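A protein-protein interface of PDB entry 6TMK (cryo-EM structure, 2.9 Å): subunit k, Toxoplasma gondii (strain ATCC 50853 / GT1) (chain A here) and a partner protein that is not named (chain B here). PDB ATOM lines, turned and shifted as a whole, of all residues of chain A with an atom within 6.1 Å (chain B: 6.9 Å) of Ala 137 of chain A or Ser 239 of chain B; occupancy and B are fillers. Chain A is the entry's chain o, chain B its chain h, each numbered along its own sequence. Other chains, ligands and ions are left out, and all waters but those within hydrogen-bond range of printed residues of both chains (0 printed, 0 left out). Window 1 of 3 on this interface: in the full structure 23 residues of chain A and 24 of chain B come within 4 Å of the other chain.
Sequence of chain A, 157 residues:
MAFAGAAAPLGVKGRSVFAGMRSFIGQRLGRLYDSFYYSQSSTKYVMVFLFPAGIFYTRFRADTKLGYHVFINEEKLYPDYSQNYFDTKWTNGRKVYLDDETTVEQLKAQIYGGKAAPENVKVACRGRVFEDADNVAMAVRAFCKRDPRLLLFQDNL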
ATOM      1  N   LEU A  66      18.093  35.837   0.399  1.00  0.00           N
ATOM      2  CA  LEU A  66      18.591  35.032  -0.704  1.00  0.00           C
ATOM      3  C   LEU A  66      17.448  34.768  -1.668  1.00  0.00           C
ATOM      4  O   LEU A  66      16.356  34.380  -1.245  1.00  0.00           O
ATOM      5  CB  LEU A  66      19.212  33.736  -0.174  1.00  0.00           C
ATOM      6  CG  LEU A  66      18.307  32.625   0.331  1.00  0.00           C
ATOM      7  CD1 LEU A  66      19.154  31.422   0.562  1.00  0.00           C
ATOM      8  CD2 LEU A  66      17.602  33.006   1.599  1.00  0.00           C
ATOM      9  N   TYR A  68      15.817  33.734  -5.825  1.00  0.00           N
ATOM     10  CA  TYR A  68      15.733  32.661  -6.798  1.00  0.00           C
ATOM     11  C   TYR A  68      15.053  33.158  -8.059  1.00  0.00           C
ATOM     12  O   TYR A  68      14.081  33.912  -7.991  1.00  0.00           O
ATOM     13  CB  TYR A  68      14.958  31.473  -6.234  1.00  0.00           C
ATOM     14  CG  TYR A  68      15.427  31.017  -4.881  1.00  0.00           C
ATOM     15  CD1 TYR A  68      16.374  30.022  -4.757  1.00  0.00           C
ATOM     16  CD2 TYR A  68      14.925  31.585  -3.728  1.00  0.00           C
ATOM     17  CE1 TYR A  68      16.804  29.606  -3.528  1.00  0.00           C
ATOM     18  CE2 TYR A  68      15.352  31.175  -2.495  1.00  0.00           C
ATOM     19  CZ  TYR A  68      16.292  30.185  -2.399  1.00  0.00           C
ATOM     20  OH  TYR A  68      16.719  29.773  -1.165  1.00  0.00           O
ATOM     21  N   ASP A  99      12.509  33.630   2.551  1.00  0.00           N
ATOM     22  CA  ASP A  99      13.098  33.395   3.856  1.00  0.00           C
ATOM     23  C   ASP A  99      13.622  31.966   3.943  1.00  0.00           C
ATOM     24  O   ASP A  99      13.245  31.089   3.165  1.00  0.00           O
ATOM     25  CB  ASP A  99      12.075  33.651   4.957  1.00  0.00           C
ATOM     26  CG  ASP A  99      11.403  34.997   4.822  1.00  0.00           C
ATOM     27  OD1 ASP A  99      10.277  35.050   4.286  1.00  0.00           O
ATOM     28  OD2 ASP A  99      11.999  36.007   5.252  1.00  0.00           O
ATOM     29  N   ASP A 100      14.507  31.744   4.914  1.00  0.00           N
ATOM     30  CA  ASP A 100      15.180  30.458   5.024  1.00  0.00           C
ATOM     31  C   ASP A 100      14.217  29.341   5.403  1.00  0.00           C
ATOM     32  O   ASP A 100      14.471  28.174   5.092  1.00  0.00           O
ATOM     33  CB  ASP A 100      16.304  30.555   6.048  1.00  0.00           C
ATOM     34  CG  ASP A 100      17.389  31.525   5.630  1.00  0.00           C
ATOM     35  OD1 ASP A 100      17.345  32.007   4.479  1.00  0.00           O
ATOM     36  OD2 ASP A 100      18.281  31.809   6.456  1.00  0.00           O
ATOM     37  N   THR A 102      11.191  28.979   4.262  1.00  0.00           N
ATOM     38  CA  THR A 102      10.182  28.787   3.232  1.00  0.00           C
ATOM     39  C   THR A 102      10.227  27.368   2.681  1.00  0.00           C
ATOM     40  O   THR A 102      11.300  26.788   2.494  1.00  0.00           O
ATOM     41  CB  THR A 102      10.394  29.789   2.102  1.00  0.00           C
ATOM     42  OG1 THR A 102      10.501  31.108   2.646  1.00  0.00           O
ATOM     43  CG2 THR A 102       9.251  29.746   1.125  1.00  0.00           C
ATOM     44  N   ASN A 135      12.612  22.208   2.516  1.00  0.00           N
ATOM     45  CA  ASN A 135      13.079  23.581   2.591  1.00  0.00           C
ATOM     46  C   ASN A 135      13.782  23.957   1.297  1.00  0.00           C
ATOM     47  O   ASN A 135      14.686  23.252   0.840  1.00  0.00           O
ATOM     48  CB  ASN A 135      14.022  23.745   3.780  1.00  0.00           C
ATOM     49  CG  ASN A 135      14.494  25.161   3.960  1.00  0.00           C
ATOM     50  OD1 ASN A 135      15.689  25.423   4.051  1.00  0.00           O
ATOM     51  ND2 ASN A 135      13.556  26.086   4.033  1.00  0.00           N
ATOM     52  N   VAL A 136      13.348  25.061   0.690  1.00  0.00           N
ATOM     53  CA  VAL A 136      13.879  25.440  -0.613  1.00  0.00           C
ATOM     54  C   VAL A 136      15.372  25.702  -0.523  1.00  0.00           C
ATOM     55  O   VAL A 136      16.139  25.338  -1.422  1.00  0.00           O
ATOM     56  CB  VAL A 136      13.125  26.670  -1.146  1.00  0.00           C
ATOM     57  CG1 VAL A 136      13.786  27.192  -2.390  1.00  0.00           C
ATOM     58  CG2 VAL A 136      11.700  26.328  -1.418  1.00  0.00           C
ATOM     59  N   ALA A 137      15.811  26.317   0.572  1.00  0.00           N
ATOM     60  CA  ALA A 137      17.217  26.664   0.719  1.00  0.00           C
ATOM     61  C   ALA A 137      18.091  25.421   0.734  1.00  0.00           C
ATOM     62  O   ALA A 137      19.085  25.336   0.003  1.00  0.00           O
ATOM     63  CB  ALA A 137      17.411  27.482   1.991  1.00  0.00           C
ATOM     64  N   MET A 138      17.732  24.438   1.558  1.00  0.00           N
ATOM     65  CA  MET A 138      18.539  23.232   1.658  1.00  0.00           C
ATOM     66  C   MET A 138      18.427  22.387   0.400  1.00  0.00           C
ATOM     67  O   MET A 138      19.404  21.756  -0.020  1.00  0.00           O
ATOM     68  CB  MET A 138      18.111  22.428   2.879  1.00  0.00           C
ATOM     69  CG  MET A 138      18.042  23.214   4.168  1.00  0.00           C
ATOM     70  SD  MET A 138      19.373  24.400   4.368  1.00  0.00           S
ATOM     71  CE  MET A 138      20.676  23.291   4.859  1.00  0.00           C
ATOM     72  N   ALA A 139      17.248  22.363  -0.220  1.00  0.00           N
ATOM     73  CA  ALA A 139      17.096  21.630  -1.470  1.00  0.00           C
ATOM     74  C   ALA A 139      17.981  22.215  -2.559  1.00  0.00           C
ATOM     75  O   ALA A 139      18.571  21.476  -3.352  1.00  0.00           O
ATOM     76  CB  ALA A 139      15.637  21.635  -1.901  1.00  0.00           C
ATOM     77  N   VAL A 140      18.083  23.541  -2.617  1.00  0.00           N
ATOM     78  CA  VAL A 140      18.955  24.174  -3.597  1.00  0.00           C
ATOM     79  C   VAL A 140      20.412  23.912  -3.254  1.00  0.00           C
ATOM     80  O   VAL A 140      21.224  23.600  -4.130  1.00  0.00           O
ATOM     81  CB  VAL A 140      18.646  25.678  -3.679  1.00  0.00           C
ATOM     82  CG1 VAL A 140      19.732  26.406  -4.433  1.00  0.00           C
ATOM     83  CG2 VAL A 140      17.310  25.897  -4.327  1.00  0.00           C
ATOM     84  N   ARG A 141      20.761  24.016  -1.972  1.00  0.00           N
ATOM     85  CA  ARG A 141      22.111  23.696  -1.530  1.00  0.00           C
ATOM     86  C   ARG A 141      22.517  22.297  -1.965  1.00  0.00           C
ATOM     87  O   ARG A 141      23.665  22.066  -2.364  1.00  0.00           O
ATOM     88  CB  ARG A 141      22.184  23.827  -0.013  1.00  0.00           C
ATOM     89  CG  ARG A 141      23.561  23.781   0.573  1.00  0.00           C
ATOM     90  CD  ARG A 141      23.467  23.684   2.070  1.00  0.00           C
ATOM     91  NE  ARG A 141      24.691  24.099   2.750  1.00  0.00           N
ATOM     92  CZ  ARG A 141      25.653  23.269   3.138  1.00  0.00           C
ATOM     93  NH1 ARG A 141      25.556  21.968   2.915  1.00  0.00           N
ATOM     94  NH2 ARG A 141      26.719  23.744   3.752  1.00  0.00           N
ATOM     95  N   ALA A 142      21.588  21.348  -1.895  1.00  0.00           N
ATOM     96  CA  ALA A 142      21.887  19.976  -2.274  1.00  0.00           C
ATOM     97  C   ALA A 142      21.958  19.812  -3.787  1.00  0.00           C
ATOM     98  O   ALA A 142      22.968  19.348  -4.325  1.00  0.00           O
ATOM     99  CB  ALA A 142      20.833  19.042  -1.692  1.00  0.00           C
ATOM    100  N   LYS A 145      23.747  23.886  -6.266  1.00  0.00           N
ATOM    101  CA  LYS A 145      24.554  24.794  -5.467  1.00  0.00           C
ATOM    102  C   LYS A 145      24.961  25.990  -6.315  1.00  0.00           C
ATOM    103  O   LYS A 145      25.641  25.834  -7.333  1.00  0.00           O
ATOM    104  CB  LYS A 145      25.781  24.057  -4.942  1.00  0.00           C
ATOM    105  CG  LYS A 145      26.579  24.775  -3.880  1.00  0.00           C
ATOM    106  CD  LYS A 145      25.866  24.776  -2.559  1.00  0.00           C
ATOM    107  CE  LYS A 145      26.840  24.879  -1.403  1.00  0.00           C
ATOM    108  NZ  LYS A 145      27.610  26.139  -1.410  1.00  0.00           N
ATOM    109  N   ARG A 146      24.548  27.183  -5.894  1.00  0.00           N
ATOM    110  CA  ARG A 146      24.900  28.438  -6.543  1.00  0.00           C
ATOM    111  C   ARG A 146      24.320  28.554  -7.947  1.00  0.00           C
ATOM    112  O   ARG A 146      24.839  29.311  -8.771  1.00  0.00           O
ATOM    113  CB  ARG A 146      26.418  28.621  -6.585  1.00  0.00           C
ATOM    114  CG  ARG A 146      27.056  28.668  -5.216  1.00  0.00           C
ATOM    115  CD  ARG A 146      28.561  28.618  -5.298  1.00  0.00           C
ATOM    116  NE  ARG A 146      29.123  29.791  -5.950  1.00  0.00           N
ATOM    117  CZ  ARG A 146      29.360  30.946  -5.340  1.00  0.00           C
ATOM    118  NH1 ARG A 146      29.869  31.955  -6.025  1.00  0.00           N
ATOM    119  NH2 ARG A 146      29.094  31.095  -4.052  1.00  0.00           N
ATOM    120  N   GLU B 220      31.119  24.716   7.664  1.00  0.00           N
ATOM    121  CA  GLU B 220      31.596  25.754   6.769  1.00  0.00           C
ATOM    122  C   GLU B 220      32.480  26.735   7.521  1.00  0.00           C
ATOM    123  O   GLU B 220      32.231  27.054   8.686  1.00  0.00           O
ATOM    124  CB  GLU B 220      30.423  26.488   6.130  1.00  0.00           C
ATOM    125  CG  GLU B 220      29.745  25.713   5.033  1.00  0.00           C
ATOM    126  CD  GLU B 220      28.718  26.534   4.290  1.00  0.00           C
ATOM    127  OE1 GLU B 220      28.833  27.778   4.299  1.00  0.00           O
ATOM    128  OE2 GLU B 220      27.795  25.937   3.698  1.00  0.00           O
ATOM    129  N   GLN B 237      23.481  36.320  -1.631  1.00  0.00           N
ATOM    130  CA  GLN B 237      23.521  35.212  -0.694  1.00  0.00           C
ATOM    131  C   GLN B 237      23.101  33.923  -1.382  1.00  0.00           C
ATOM    132  O   GLN B 237      22.096  33.885  -2.097  1.00  0.00           O
ATOM    133  CB  GLN B 237      22.612  35.494   0.497  1.00  0.00           C
ATOM    134  CG  GLN B 237      23.029  36.687   1.314  1.00  0.00           C
ATOM    135  CD  GLN B 237      24.302  36.453   2.087  1.00  0.00           C
ATOM    136  OE1 GLN B 237      24.334  35.670   3.034  1.00  0.00           O
ATOM    137  NE2 GLN B 237      25.363  37.140   1.693  1.00  0.00           N
ATOM    138  N   TYR B 238      23.882  32.874  -1.162  1.00  0.00           N
ATOM    139  CA  TYR B 238      23.645  31.559  -1.729  1.00  0.00           C
ATOM    140  C   TYR B 238      23.491  30.552  -0.602  1.00  0.00           C
ATOM    141  O   TYR B 238      24.206  30.608   0.402  1.00  0.00           O
ATOM    142  CB  TYR B 238      24.775  31.158  -2.670  1.00  0.00           C
ATOM    143  CG  TYR B 238      24.845  32.028  -3.899  1.00  0.00           C
ATOM    144  CD1 TYR B 238      23.812  32.035  -4.819  1.00  0.00           C
ATOM    145  CD2 TYR B 238      25.925  32.858  -4.128  1.00  0.00           C
ATOM    146  CE1 TYR B 238      23.859  32.830  -5.935  1.00  0.00           C
ATOM    147  CE2 TYR B 238      25.981  33.658  -5.247  1.00  0.00           C
ATOM    148  CZ  TYR B 238      24.941  33.643  -6.142  1.00  0.00           C
ATOM    149  OH  TYR B 238      24.991  34.440  -7.259  1.00  0.00           O
ATOM    150  N   SER B 239      22.545  29.641  -0.781  1.00  0.00           N
ATOM    151  CA  SER B 239      22.202  28.650   0.224  1.00  0.00           C
ATOM    152  C   SER B 239      23.405  27.802   0.621  1.00  0.00           C
ATOM    153  O   SER B 239      23.487  27.317   1.749  1.00  0.00           O
ATOM    154  CB  SER B 239      21.085  27.760  -0.310  1.00  0.00           C
ATOM    155  OG  SER B 239      19.991  28.544  -0.746  1.00  0.00           O
ATOM    156  OXT SER B 239      24.321  27.585  -0.171  1.00  0.00           O
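The side-chain carboxylate (OE2) of Glu 220 of chain B is in salt-bridge range of the guanidinium group (NH2) of Arg 141 of chain A. The side-chain hydroxyl of Ser 239 of chain B lies close to the backbone carbonyl oxygen of Ala 137 of chain A (3.4 Å). The chain-end carboxylate (O) of Ser 239 of chain B is in salt-bridge range of the guanidinium group (NE) of Arg 141 of chain A. NZ of Lys 145 of chain A is in salt-bridge range of OXT of Ser 239 of chain B.
Of the printed residues of chain B, Leu 66 of chain A touches Gln 237 (3.5 Å) and Ser 239 (3.3 Å). Printed residues of chain B within 4 Å of Tyr 68 of chain A: Ser 239 (3.5 Å). Asn 135 of chain A touches none of the printed residues of chain B. Val 136 of chain A touches none of the printed residues of chain B. Ala 137 of chain A touches just one residue of chain B: Ser 239 (3.2 Å). Printed residues of chain B within 4 Å of Arg 141 of chain A: Glu 220 and Ser 239. Of the printed residues of chain B, Lys 145 of chain A touches Ser 239. Ser 239 of chain B touches just these residues of chain A: Leu 66 (3.3 Å), Tyr 68 (3.5 Å), Ala 137 (3.2 Å), Arg 141 (3.6 Å) and Lys 145 (3.8 Å). The nearest printed residue of chain B that does not touch Ala 137 of chain A is Tyr 238 of chain B (6.9 Å). The nearest residue of chain A that does not touch Ser 239 of chain B is Val 140 of chain A (4.3 Å). The nearest printed residue of chain B that does not touch Lys 145 of chain A is Glu 220 of chain B (5.1 Å).
Among the printed residues, Asp or Glu carboxylates within 4 Å of a Lys or Arg side-chain nitrogen of the other chain: Arg 141 of chain A with Glu 220 of chain B (2.4 Å).
Among the printed residues, pairs that only touch across the chains: Leu 66 of chain A with Ser 239 of chain B, Leu 66 of chain A with Gln 237 of chain B, Tyr 68 of chain A with Ser 239 of chain B and Arg 146 of chain A with Tyr 238 of chain B.
O of Val 140 of chain A lies within hydrogen-bond range of N of Lys 145 of chain A.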
